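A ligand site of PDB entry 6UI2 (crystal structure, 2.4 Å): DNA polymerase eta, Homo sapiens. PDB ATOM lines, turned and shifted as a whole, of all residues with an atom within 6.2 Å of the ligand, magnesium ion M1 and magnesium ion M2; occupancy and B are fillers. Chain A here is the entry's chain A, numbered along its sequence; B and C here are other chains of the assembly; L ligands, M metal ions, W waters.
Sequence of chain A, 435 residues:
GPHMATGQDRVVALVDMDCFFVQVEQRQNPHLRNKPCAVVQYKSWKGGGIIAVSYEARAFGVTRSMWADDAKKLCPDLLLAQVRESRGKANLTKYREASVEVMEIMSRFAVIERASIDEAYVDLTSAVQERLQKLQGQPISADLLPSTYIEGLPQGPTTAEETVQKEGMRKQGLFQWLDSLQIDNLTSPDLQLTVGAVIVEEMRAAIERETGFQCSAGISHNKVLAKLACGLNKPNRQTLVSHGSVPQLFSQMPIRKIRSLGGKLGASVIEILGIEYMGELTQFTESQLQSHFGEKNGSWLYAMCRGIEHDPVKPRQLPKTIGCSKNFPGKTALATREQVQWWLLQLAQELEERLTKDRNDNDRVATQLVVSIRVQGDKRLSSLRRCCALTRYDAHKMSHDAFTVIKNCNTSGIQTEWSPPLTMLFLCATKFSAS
Water W3 lies within hydrogen-bond range of O4 of the ligand (2.7 Å), N of Val 53 (2.9 Å) and NH2 of Arg 58 (3.0 Å). Water W1 bridges O1 of the ligand (2.9 Å) and NH2 of Arg 64 (3.2 Å).
An oxygen (O11) of the ligand lies within hydrogen-bond range of the backbone NH (N) of Phe 21 (3.2 Å). N of Cys 19 sits at hydrogen-bond distance from O3 of the ligand. NH1 of Arg 58 lies within salt-bridge range of O1 of the ligand (3.0 Å). OH of Tyr 55 lies within hydrogen-bond range of O3 of the ligand, at 2.8 Å. The backbone NH (N) of Phe 20 sits at hydrogen-bond distance from an oxygen (O11) of the ligand. N3 of DT 8 of chain B sits close to N4 of the ligand (3.4 Å). The guanidinium group (NH2) of Arg 64 lies within salt-bridge range of an oxygen (O4) of the ligand. O6 of FMG 4 of chain C lies within hydrogen-bond range of a nitrogen (N4) of the ligand. The side-chain amino group of Lys 234 lies within salt-bridge range of an oxygen (O3) of the ligand, at 3.3 Å.
Magnesium ion M1 is bound by an oxygen (O2) of the ligand (2.0 Å), the side-chain carboxylate of Asp 16 (2.0 Å), the backbone carbonyl oxygen of Met 17 (2.1 Å), an oxygen (O5) of the ligand (2.1 Å), the side-chain carboxylate of Asp 118 (2.2 Å) and an oxygen (O7) of the ligand (2.3 Å).
Merely in contact with the ligand: Asp 18, Ile 51, Ala 52 and Ile 117. Hydrophobic or aromatic side chains within 4 Å of the ligand: Phe 20, Phe 21, Ala 52, Tyr 55 and Ile 117. Within 4 Å of the ligand: Asp 16, Met 17, Asp 18, Cys 19, Phe 20, Phe 21, Ile 51, Ala 52, Tyr 55, Arg 58, Arg 64, Ile 117, Asp 118, Glu 119, Lys 234, DT 8 of chain B and FMG 4 of chain C. The nearest printed residue that does not touch the ligand is DA 5 of chain C (4.02 Å).
NZ of Lys 234 touches magnesium ion M1, 3.8 Å away. Of the 25 residues printed, 4 come within 4 Å of magnesium ion M1. The nearest printed residue that does not touch magnesium ion M1 is Asp 18 (4.3 Å).
Magnesium ion M2 is bound by OE1 of Glu 119, 1.9 Å away. O7 of the ligand binds magnesium ion M2, at 2.1 Å. The side-chain carboxylate (OD2) of Asp 16 binds magnesium ion M2, 2.2 Å away. Magnesium ion M2 is bound by O3' of DT 8 of chain B (2.2 Å). Magnesium ion M2 is bound by the side-chain carboxylate (OD1) of Asp 118 (2.2 Å).
O of Met 17 lies close to NZ of Lys 234 (3.4 Å). The side-chain carboxylate (OE2) of Glu 119 is in salt-bridge range of the side-chain amino group (NZ) of Lys 227 (2.6 Å). OH of Tyr 55 is in hydrogen-bond range of NH1 of Arg 58 (3.0 Å). OD1 of Asp 18 is in salt-bridge range of NZ of Lys 234, 2.8 Å away. O of Asp 16 lies within hydrogen-bond range of NZ of Lys 234, at 3.2 Å. The guanidinium group (NE) of Arg 58 is in hydrogen-bond range of the backbone carbonyl oxygen (O) of Val 53, 3.0 Å away. OG of Ser 116 sits close to O3' of DT 8 of chain B (3.2 Å). The backbone NH (N) of Asp 118 sits close to the side-chain hydroxyl (OG) of Ser 116, 3.1 Å away.
Ser 116 touches magnesium ion M2. The nearest printed residue that does not touch magnesium ion M2 is Lys 227 (4.2 Å).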
ATOM      1  N   ASP A  16      13.319  16.770   1.165  1.00  0.00           N
ATOM      2  CA  ASP A  16      13.817  17.056   2.494  1.00  0.00           C
ATOM      3  C   ASP A  16      13.721  15.814   3.365  1.00  0.00           C
ATOM      4  O   ASP A  16      12.661  15.193   3.449  1.00  0.00           O
ATOM      5  CB  ASP A  16      13.028  18.216   3.110  1.00  0.00           C
ATOM      6  CG  ASP A  16      13.580  18.649   4.432  1.00  0.00           C
ATOM      7  OD1 ASP A  16      13.288  17.974   5.419  1.00  0.00           O
ATOM      8  OD2 ASP A  16      14.362  19.616   4.474  1.00  0.00           O
ATOM      9  N   MET A  17      14.826  15.446   4.007  1.00  0.00           N
ATOM     10  CA  MET A  17      14.864  14.219   4.783  1.00  0.00           C
ATOM     11  C   MET A  17      14.054  14.368   6.067  1.00  0.00           C
ATOM     12  O   MET A  17      14.079  15.415   6.721  1.00  0.00           O
ATOM     13  CB  MET A  17      16.305  13.836   5.108  1.00  0.00           C
ATOM     14  CG  MET A  17      17.255  13.943   3.879  1.00  0.00           C
ATOM     15  SD  MET A  17      16.767  12.871   2.485  1.00  0.00           S
ATOM     16  CE  MET A  17      16.761  11.302   3.317  1.00  0.00           C
ATOM     17  N   ASP A  18      13.291  13.332   6.389  1.00  0.00           N
ATOM     18  CA  ASP A  18      12.532  13.320   7.640  1.00  0.00           C
ATOM     19  C   ASP A  18      13.485  13.125   8.813  1.00  0.00           C
ATOM     20  O   ASP A  18      14.330  12.217   8.777  1.00  0.00           O
ATOM     21  CB  ASP A  18      11.458  12.218   7.595  1.00  0.00           C
ATOM     22  CG  ASP A  18      10.480  12.390   6.426  1.00  0.00           C
ATOM     23  OD1 ASP A  18      10.295  13.546   5.988  1.00  0.00           O
ATOM     24  OD2 ASP A  18       9.899  11.387   5.935  1.00  0.00           O
ATOM     25  N   CYS A  19      13.344  13.971   9.841  1.00  0.00           N
ATOM     26  CA  CYS A  19      14.168  13.938  11.060  1.00  0.00           C
ATOM     27  C   CYS A  19      15.580  13.423  10.775  1.00  0.00           C
ATOM     28  O   CYS A  19      15.994  12.410  11.347  1.00  0.00           O
ATOM     29  CB  CYS A  19      13.478  13.117  12.151  1.00  0.00           C
ATOM     30  SG  CYS A  19      12.924  11.469  11.662  1.00  0.00           S
ATOM     31  N   PHE A  20      16.313  14.122   9.909  1.00  0.00           N
ATOM     32  CA  PHE A  20      17.484  13.548   9.253  1.00  0.00           C
ATOM     33  C   PHE A  20      18.512  12.986  10.229  1.00  0.00           C
ATOM     34  O   PHE A  20      18.890  11.814  10.130  1.00  0.00           O
ATOM     35  CB  PHE A  20      18.156  14.592   8.357  1.00  0.00           C
ATOM     36  CG  PHE A  20      19.309  14.043   7.578  1.00  0.00           C
ATOM     37  CD1 PHE A  20      19.176  12.847   6.884  1.00  0.00           C
ATOM     38  CD2 PHE A  20      20.526  14.698   7.552  1.00  0.00           C
ATOM     39  CE1 PHE A  20      20.223  12.322   6.157  1.00  0.00           C
ATOM     40  CE2 PHE A  20      21.608  14.176   6.816  1.00  0.00           C
ATOM     41  CZ  PHE A  20      21.446  12.987   6.123  1.00  0.00           C
ATOM     42  N   PHE A  21      19.008  13.815  11.166  1.00  0.00           N
ATOM     43  CA  PHE A  21      20.052  13.328  12.075  1.00  0.00           C
ATOM     44  C   PHE A  21      19.578  12.127  12.892  1.00  0.00           C
ATOM     45  O   PHE A  21      20.373  11.228  13.172  1.00  0.00           O
ATOM     46  CB  PHE A  21      20.556  14.422  13.016  1.00  0.00           C
ATOM     47  CG  PHE A  21      21.388  15.509  12.342  1.00  0.00           C
ATOM     48  CD1 PHE A  21      21.410  15.663  10.961  1.00  0.00           C
ATOM     49  CD2 PHE A  21      22.139  16.379  13.103  1.00  0.00           C
ATOM     50  CE1 PHE A  21      22.161  16.686  10.349  1.00  0.00           C
ATOM     51  CE2 PHE A  21      22.905  17.393  12.491  1.00  0.00           C
ATOM     52  CZ  PHE A  21      22.906  17.546  11.118  1.00  0.00           C
ATOM     53  N   VAL A  22      18.282  12.064  13.231  1.00  0.00           N
ATOM     54  CA  VAL A  22      17.737  10.901  13.918  1.00  0.00           C
ATOM     55  C   VAL A  22      17.772   9.661  13.013  1.00  0.00           C
ATOM     56  O   VAL A  22      18.157   8.568  13.439  1.00  0.00           O
ATOM     57  CB  VAL A  22      16.316  11.188  14.438  1.00  0.00           C
ATOM     58  CG1 VAL A  22      15.654   9.918  14.917  1.00  0.00           C
ATOM     59  CG2 VAL A  22      16.368  12.182  15.595  1.00  0.00           C
ATOM     60  N   ILE A  51      18.846  18.620  18.914  1.00  0.00           N
ATOM     61  CA  ILE A  51      18.932  19.191  17.573  1.00  0.00           C
ATOM     62  C   ILE A  51      18.144  18.418  16.539  1.00  0.00           C
ATOM     63  O   ILE A  51      17.991  18.904  15.415  1.00  0.00           O
ATOM     64  CB  ILE A  51      20.400  19.363  17.119  1.00  0.00           C
ATOM     65  CG1 ILE A  51      21.091  18.019  16.965  1.00  0.00           C
ATOM     66  CG2 ILE A  51      21.169  20.259  18.096  1.00  0.00           C
ATOM     67  CD1 ILE A  51      22.582  18.161  16.584  1.00  0.00           C
ATOM     68  N   ALA A  52      17.604  17.236  16.858  1.00  0.00           N
ATOM     69  CA  ALA A  52      16.706  16.563  15.926  1.00  0.00           C
ATOM     70  C   ALA A  52      15.833  15.595  16.710  1.00  0.00           C
ATOM     71  O   ALA A  52      16.294  14.996  17.681  1.00  0.00           O
ATOM     72  CB  ALA A  52      17.470  15.829  14.806  1.00  0.00           C
ATOM     73  N   VAL A  53      14.564  15.453  16.301  1.00  0.00           N
ATOM     74  CA  VAL A  53      13.534  14.738  17.064  1.00  0.00           C
ATOM     75  C   VAL A  53      12.754  13.825  16.132  1.00  0.00           C
ATOM     76  O   VAL A  53      12.199  14.289  15.133  1.00  0.00           O
ATOM     77  CB  VAL A  53      12.562  15.711  17.734  1.00  0.00           C
ATOM     78  CG1 VAL A  53      11.686  14.969  18.727  1.00  0.00           C
ATOM     79  CG2 VAL A  53      13.272  16.878  18.377  1.00  0.00           C
ATOM     80  N   TYR A  55       9.534  11.597  14.845  1.00  0.00           N
ATOM     81  CA  TYR A  55       8.104  11.909  14.877  1.00  0.00           C
ATOM     82  C   TYR A  55       7.398  11.227  16.046  1.00  0.00           C
ATOM     83  O   TYR A  55       6.449  11.784  16.592  1.00  0.00           O
ATOM     84  CB  TYR A  55       7.444  11.543  13.539  1.00  0.00           C
ATOM     85  CG  TYR A  55       7.755  12.599  12.499  1.00  0.00           C
ATOM     86  CD1 TYR A  55       8.955  12.592  11.810  1.00  0.00           C
ATOM     87  CD2 TYR A  55       6.890  13.659  12.275  1.00  0.00           C
ATOM     88  CE1 TYR A  55       9.255  13.570  10.894  1.00  0.00           C
ATOM     89  CE2 TYR A  55       7.174  14.644  11.359  1.00  0.00           C
ATOM     90  CZ  TYR A  55       8.370  14.606  10.667  1.00  0.00           C
ATOM     91  OH  TYR A  55       8.682  15.605   9.748  1.00  0.00           O
ATOM     92  N   ARG A  58       7.975  13.672  18.693  1.00  0.00           N
ATOM     93  CA  ARG A  58       7.225  14.906  18.464  1.00  0.00           C
ATOM     94  C   ARG A  58       5.804  14.796  18.972  1.00  0.00           C
ATOM     95  O   ARG A  58       5.224  15.807  19.387  1.00  0.00           O
ATOM     96  CB  ARG A  58       7.209  15.278  16.981  1.00  0.00           C
ATOM     97  CG  ARG A  58       8.597  15.590  16.415  1.00  0.00           C
ATOM     98  CD  ARG A  58       8.580  16.129  14.984  1.00  0.00           C
ATOM     99  NE  ARG A  58       9.905  16.016  14.393  1.00  0.00           N
ATOM    100  CZ  ARG A  58      10.249  16.386  13.161  1.00  0.00           C
ATOM    101  NH1 ARG A  58       9.354  16.931  12.343  1.00  0.00           N
ATOM    102  NH2 ARG A  58      11.502  16.205  12.760  1.00  0.00           N
ATOM    103  N   ARG A  64      13.119  20.499  18.961  1.00  0.00           N
ATOM    104  CA  ARG A  64      14.469  21.048  18.840  1.00  0.00           C
ATOM    105  C   ARG A  64      14.641  22.200  19.822  1.00  0.00           C
ATOM    106  O   ARG A  64      13.655  22.808  20.229  1.00  0.00           O
ATOM    107  CB  ARG A  64      14.696  21.492  17.385  1.00  0.00           C
ATOM    108  CG  ARG A  64      15.952  22.310  17.138  1.00  0.00           C
ATOM    109  CD  ARG A  64      16.045  22.809  15.684  1.00  0.00           C
ATOM    110  NE  ARG A  64      15.905  21.705  14.730  1.00  0.00           N
ATOM    111  CZ  ARG A  64      14.861  21.535  13.919  1.00  0.00           C
ATOM    112  NH1 ARG A  64      13.866  22.421  13.915  1.00  0.00           N
ATOM    113  NH2 ARG A  64      14.838  20.489  13.094  1.00  0.00           N
ATOM    114  N   LEU A  92      30.169  17.096  13.226  1.00  0.00           N
ATOM    115  CA  LEU A  92      28.984  16.693  12.479  1.00  0.00           C
ATOM    116  C   LEU A  92      29.323  15.856  11.238  1.00  0.00           C
ATOM    117  O   LEU A  92      28.468  15.681  10.366  1.00  0.00           O
ATOM    118  CB  LEU A  92      28.153  17.921  12.098  1.00  0.00           C
ATOM    119  CG  LEU A  92      27.649  18.744  13.300  1.00  0.00           C
ATOM    120  CD1 LEU A  92      26.929  19.957  12.843  1.00  0.00           C
ATOM    121  CD2 LEU A  92      26.753  17.940  14.209  1.00  0.00           C
ATOM    122  N   SER A 116      20.534  22.566   2.011  1.00  0.00           N
ATOM    123  CA  SER A 116      20.948  22.413   3.403  1.00  0.00           C
ATOM    124  C   SER A 116      21.598  21.043   3.519  1.00  0.00           C
ATOM    125  O   SER A 116      21.715  20.310   2.535  1.00  0.00           O
ATOM    126  CB  SER A 116      19.754  22.542   4.363  1.00  0.00           C
ATOM    127  OG  SER A 116      19.014  21.316   4.413  1.00  0.00           O
ATOM    128  N   ILE A 117      21.995  20.667   4.738  1.00  0.00           N
ATOM    129  CA  ILE A 117      22.570  19.342   4.881  1.00  0.00           C
ATOM    130  C   ILE A 117      21.575  18.234   4.519  1.00  0.00           C
ATOM    131  O   ILE A 117      21.989  17.114   4.212  1.00  0.00           O
ATOM    132  CB  ILE A 117      23.115  19.127   6.308  1.00  0.00           C
ATOM    133  CG1 ILE A 117      24.118  17.979   6.320  1.00  0.00           C
ATOM    134  CG2 ILE A 117      21.993  18.872   7.294  1.00  0.00           C
ATOM    135  CD1 ILE A 117      24.951  17.905   7.614  1.00  0.00           C
ATOM    136  N   ASP A 118      20.268  18.529   4.538  1.00  0.00           N
ATOM    137  CA  ASP A 118      19.271  17.469   4.334  1.00  0.00           C
ATOM    138  C   ASP A 118      18.225  17.819   3.291  1.00  0.00           C
ATOM    139  O   ASP A 118      17.158  17.174   3.250  1.00  0.00           O
ATOM    140  CB  ASP A 118      18.598  17.101   5.664  1.00  0.00           C
ATOM    141  CG  ASP A 118      17.259  17.820   5.878  1.00  0.00           C
ATOM    142  OD1 ASP A 118      17.210  19.069   5.692  1.00  0.00           O
ATOM    143  OD2 ASP A 118      16.268  17.113   6.211  1.00  0.00           O
ATOM    144  N   GLU A 119      18.477  18.795   2.414  1.00  0.00           N
ATOM    145  CA  GLU A 119      17.491  19.062   1.370  1.00  0.00           C
ATOM    146  C   GLU A 119      18.121  19.678   0.135  1.00  0.00           C
ATOM    147  O   GLU A 119      19.184  20.305   0.200  1.00  0.00           O
ATOM    148  CB  GLU A 119      16.348  19.949   1.903  1.00  0.00           C
ATOM    149  CG  GLU A 119      16.623  21.422   2.014  1.00  0.00           C
ATOM    150  CD  GLU A 119      15.910  22.020   3.234  1.00  0.00           C
ATOM    151  OE1 GLU A 119      16.221  21.593   4.364  1.00  0.00           O
ATOM    152  OE2 GLU A 119      15.026  22.890   3.062  1.00  0.00           O
ATOM    153  N   LYS A 227       9.033  24.135  -1.544  1.00  0.00           N
ATOM    154  CA  LYS A 227       9.402  24.081  -0.126  1.00  0.00           C
ATOM    155  C   LYS A 227       8.154  24.074   0.760  1.00  0.00           C
ATOM    156  O   LYS A 227       8.029  23.248   1.669  1.00  0.00           O
ATOM    157  CB  LYS A 227      10.316  25.267   0.203  1.00  0.00           C
ATOM    158  CG  LYS A 227      10.809  25.414   1.662  1.00  0.00           C
ATOM    159  CD  LYS A 227      11.450  24.118   2.183  1.00  0.00           C
ATOM    160  CE  LYS A 227      11.942  24.215   3.641  1.00  0.00           C
ATOM    161  NZ  LYS A 227      12.652  22.959   4.089  1.00  0.00           N
ATOM    162  N   LYS A 234       4.546  15.894   5.532  1.00  0.00           N
ATOM    163  CA  LYS A 234       5.580  15.147   6.209  1.00  0.00           C
ATOM    164  C   LYS A 234       4.926  14.331   7.304  1.00  0.00           C
ATOM    165  O   LYS A 234       3.935  14.763   7.867  1.00  0.00           O
ATOM    166  CB  LYS A 234       6.637  16.094   6.786  1.00  0.00           C
ATOM    167  CG  LYS A 234       7.669  16.520   5.799  1.00  0.00           C
ATOM    168  CD  LYS A 234       8.712  17.442   6.444  1.00  0.00           C
ATOM    169  CE  LYS A 234       9.989  17.489   5.609  1.00  0.00           C
ATOM    170  NZ  LYS A 234      10.858  16.280   5.850  1.00  0.00           N
ATOM    171  N   PRO A 235       5.457  13.143   7.634  1.00  0.00           N
ATOM    172  CA  PRO A 235       6.635  12.452   7.104  1.00  0.00           C
ATOM    173  C   PRO A 235       6.344  11.453   5.976  1.00  0.00           C
ATOM    174  O   PRO A 235       5.226  10.953   5.835  1.00  0.00           O
ATOM    175  CB  PRO A 235       7.153  11.706   8.338  1.00  0.00           C
ATOM    176  CG  PRO A 235       5.892  11.316   9.070  1.00  0.00           C
ATOM    177  CD  PRO A 235       4.951  12.489   8.859  1.00  0.00           C
ATOM    178  P    DT B   8      14.202  26.641   7.185  1.00  0.00           P
ATOM    179  OP1  DT B   8      13.121  26.032   6.384  1.00  0.00           O
ATOM    180  OP2  DT B   8      13.925  27.125   8.563  1.00  0.00           O
ATOM    181  O5'  DT B   8      15.401  25.589   7.303  1.00  0.00           O
ATOM    182  C5'  DT B   8      16.217  25.286   6.171  1.00  0.00           C
ATOM    183  C4'  DT B   8      17.209  24.217   6.546  1.00  0.00           C
ATOM    184  O4'  DT B   8      18.270  24.803   7.343  1.00  0.00           O
ATOM    185  C3'  DT B   8      16.605  23.094   7.382  1.00  0.00           C
ATOM    186  O3'  DT B   8      17.117  21.839   6.936  1.00  0.00           O
ATOM    187  C2'  DT B   8      17.040  23.434   8.815  1.00  0.00           C
ATOM    188  C1'  DT B   8      18.373  24.142   8.584  1.00  0.00           C
ATOM    189  N1   DT B   8      18.672  25.141   9.612  1.00  0.00           N
ATOM    190  C2   DT B   8      19.889  25.109  10.244  1.00  0.00           C
ATOM    191  O2   DT B   8      20.734  24.259   9.996  1.00  0.00           O
ATOM    192  N3   DT B   8      20.077  26.084  11.175  1.00  0.00           N
ATOM    193  C4   DT B   8      19.196  27.075  11.538  1.00  0.00           C
ATOM    194  O4   DT B   8      19.464  27.908  12.381  1.00  0.00           O
ATOM    195  C5   DT B   8      17.923  27.052  10.844  1.00  0.00           C
ATOM    196  C7   DT B   8      16.870  28.077  11.149  1.00  0.00           C
ATOM    197  C6   DT B   8      17.734  26.099   9.925  1.00  0.00           C
ATOM    198  P    DT C   3      19.091  29.464  25.990  1.00  0.00           P
ATOM    199  OP1  DT C   3      18.907  30.838  26.525  1.00  0.00           O
ATOM    200  OP2  DT C   3      17.949  28.537  25.858  1.00  0.00           O
ATOM    201  O5'  DT C   3      19.772  29.596  24.538  1.00  0.00           O
ATOM    202  C5'  DT C   3      19.340  28.750  23.471  1.00  0.00           C
ATOM    203  C4'  DT C   3      19.948  27.377  23.603  1.00  0.00           C
ATOM    204  O4'  DT C   3      19.257  26.434  22.762  1.00  0.00           O
ATOM    205  C3'  DT C   3      21.398  27.276  23.175  1.00  0.00           C
ATOM    206  O3'  DT C   3      22.282  27.591  24.271  1.00  0.00           O
ATOM    207  C2'  DT C   3      21.541  25.805  22.725  1.00  0.00           C
ATOM    208  C1'  DT C   3      20.096  25.309  22.603  1.00  0.00           C
ATOM    209  N1   DT C   3      19.799  24.634  21.294  1.00  0.00           N
ATOM    210  C2   DT C   3      20.332  23.383  21.053  1.00  0.00           C
ATOM    211  O2   DT C   3      21.042  22.804  21.842  1.00  0.00           O
ATOM    212  N3   DT C   3      19.998  22.847  19.844  1.00  0.00           N
ATOM    213  C4   DT C   3      19.210  23.425  18.852  1.00  0.00           C
ATOM    214  O4   DT C   3      18.969  22.855  17.792  1.00  0.00           O
ATOM    215  C5   DT C   3      18.683  24.735  19.164  1.00  0.00           C
ATOM    216  C7   DT C   3      17.807  25.456  18.175  1.00  0.00           C
ATOM    217  C6   DT C   3      19.000  25.279  20.359  1.00  0.00           C
ATOM    218  P   FMG C   4      23.835  27.882  23.983  1.00  0.00           P
ATOM    219  OP2 FMG C   4      23.913  28.994  22.964  1.00  0.00           O
ATOM    220  OP1 FMG C   4      24.608  27.963  25.277  1.00  0.00           O
ATOM    221  O5' FMG C   4      24.339  26.538  23.291  1.00  0.00           O
ATOM    222  F1' FMG C   4      25.255  27.411  19.029  1.00  0.00           F
ATOM    223  N9  FMG C   4      23.187  25.732  18.660  1.00  0.00           N
ATOM    224  C8  FMG C   4      22.464  26.862  18.840  1.00  0.00           C
ATOM    225  N7  FMG C   4      21.464  26.951  17.946  1.00  0.00           N
ATOM    226  CM7 FMG C   4      20.461  28.049  17.854  1.00  0.00           C
ATOM    227  C5  FMG C   4      21.538  25.854  17.193  1.00  0.00           C
ATOM    228  C4  FMG C   4      22.668  25.063  17.648  1.00  0.00           C
ATOM    229  N3  FMG C   4      22.952  23.894  17.027  1.00  0.00           N
ATOM    230  C2  FMG C   4      22.183  23.478  15.993  1.00  0.00           C
ATOM    231  N2  FMG C   4      22.532  22.309  15.404  1.00  0.00           N
ATOM    232  N1  FMG C   4      21.118  24.184  15.530  1.00  0.00           N
ATOM    233  C6  FMG C   4      20.735  25.362  16.063  1.00  0.00           C
ATOM    234  O6  FMG C   4      19.752  25.990  15.633  1.00  0.00           O
ATOM    235  C2' FMG C   4      25.585  26.083  19.129  1.00  0.00           C
ATOM    236  C5' FMG C   4      25.469  26.619  22.460  1.00  0.00           C
ATOM    237  C4' FMG C   4      25.415  25.490  21.462  1.00  0.00           C
ATOM    238  O4' FMG C   4      24.144  25.352  20.824  1.00  0.00           O
ATOM    239  C1' FMG C   4      24.363  25.242  19.405  1.00  0.00           C
ATOM    240  C3' FMG C   4      26.385  25.911  20.394  1.00  0.00           C
ATOM    241  O3' FMG C   4      27.268  24.843  20.247  1.00  0.00           O
ATOM    242  P    DA C   5      28.679  25.125  19.569  1.00  0.00           P
ATOM    243  OP1  DA C   5      29.631  24.228  20.253  1.00  0.00           O
ATOM    244  OP2  DA C   5      28.951  26.578  19.597  1.00  0.00           O
ATOM    245  O5'  DA C   5      28.437  24.667  18.053  1.00  0.00           O
ATOM    246  C5'  DA C   5      28.126  23.295  17.789  1.00  0.00           C
ATOM    247  C4'  DA C   5      27.973  23.023  16.311  1.00  0.00           C
ATOM    248  O4'  DA C   5      26.677  23.489  15.847  1.00  0.00           O
ATOM    249  C3'  DA C   5      29.013  23.705  15.423  1.00  0.00           C
ATOM    250  O3'  DA C   5      29.335  22.816  14.367  1.00  0.00           O
ATOM    251  C2'  DA C   5      28.245  24.926  14.911  1.00  0.00           C
ATOM    252  C1'  DA C   5      26.850  24.341  14.753  1.00  0.00           C
ATOM    253  N9   DA C   5      25.789  25.323  14.771  1.00  0.00           N
ATOM    254  C8   DA C   5      25.711  26.425  15.573  1.00  0.00           C
ATOM    255  N7   DA C   5      24.649  27.151  15.379  1.00  0.00           N
ATOM    256  C5   DA C   5      23.966  26.484  14.369  1.00  0.00           C
ATOM    257  C6   DA C   5      22.749  26.744  13.696  1.00  0.00           C
ATOM    258  N6   DA C   5      21.976  27.798  13.967  1.00  0.00           N
ATOM    259  N1   DA C   5      22.369  25.886  12.742  1.00  0.00           N
ATOM    260  C2   DA C   5      23.149  24.834  12.477  1.00  0.00           C
ATOM    261  N3   DA C   5      24.311  24.484  13.036  1.00  0.00           N
ATOM    262  C4   DA C   5      24.667  25.359  13.983  1.00  0.00           C
HETATM  263  P1  LIG L   1      11.882  17.178   9.330  1.00  0.00           P
HETATM  264  O1  LIG L   1      10.830  18.040   9.996  1.00  0.00           O
HETATM  265  O2  LIG L   1      12.566  17.903   8.115  1.00  0.00           O
HETATM  266  O3  LIG L   1      11.350  15.716   9.032  1.00  0.00           O
HETATM  267  P2  LIG L   1      14.572  17.060  10.287  1.00  0.00           P
HETATM  268  O4  LIG L   1      15.392  17.056  11.595  1.00  0.00           O
HETATM  269  O5  LIG L   1      15.321  17.220   8.920  1.00  0.00           O
HETATM  270  O6  LIG L   1      13.014  17.213  10.473  1.00  0.00           O
HETATM  271  P3  LIG L   1      14.948  19.909   9.091  1.00  0.00           P
HETATM  272  O7  LIG L   1      15.433  19.408   7.617  1.00  0.00           O
HETATM  273  O8  LIG L   1      15.148  21.390   9.362  1.00  0.00           O
HETATM  274  N1  LIG L   1      14.684  18.728  10.413  1.00  0.00           N
HETATM  275  O9  LIG L   1      16.598  19.882   9.398  1.00  0.00           O
HETATM  276  C1  LIG L   1      17.579  18.929   8.896  1.00  0.00           C
HETATM  277  C2  LIG L   1      18.619  18.437   9.949  1.00  0.00           C
HETATM  278  O10 LIG L   1      19.467  19.574  10.181  1.00  0.00           O
HETATM  279  C3  LIG L   1      18.029  18.134  11.324  1.00  0.00           C
HETATM  280  O11 LIG L   1      17.900  16.787  11.460  1.00  0.00           O
HETATM  281  C4  LIG L   1      19.180  18.526  12.281  1.00  0.00           C
HETATM  282  C5  LIG L   1      19.830  19.686  11.552  1.00  0.00           C
HETATM  283  N2  LIG L   1      19.348  21.009  12.024  1.00  0.00           N
HETATM  284  C6  LIG L   1      20.129  21.684  12.920  1.00  0.00           C
HETATM  285  N3  LIG L   1      19.705  22.944  13.403  1.00  0.00           N
HETATM  286  C7  LIG L   1      18.488  23.469  13.020  1.00  0.00           C
HETATM  287  C8  LIG L   1      17.657  22.775  12.108  1.00  0.00           C
HETATM  288  C9  LIG L   1      18.080  21.537  11.636  1.00  0.00           C
HETATM  289  O12 LIG L   1      21.197  21.246  13.330  1.00  0.00           O
HETATM  290  N4  LIG L   1      18.163  24.634  13.551  1.00  0.00           N
HETATM  291 MG    MG M   1      14.292  17.448   7.120  1.00  0.00          MG
HETATM  292 MG    MG M   2      15.611  20.610   5.926  1.00  0.00          MG
HETATM  293  O   HOH W   1      11.958  20.003  11.734  1.00  0.00           O
HETATM  294  O   HOH W   2      11.793  20.213   7.283  1.00  0.00           O
HETATM  295  O   HOH W   3      14.113  17.179  13.972  1.00  0.00           O
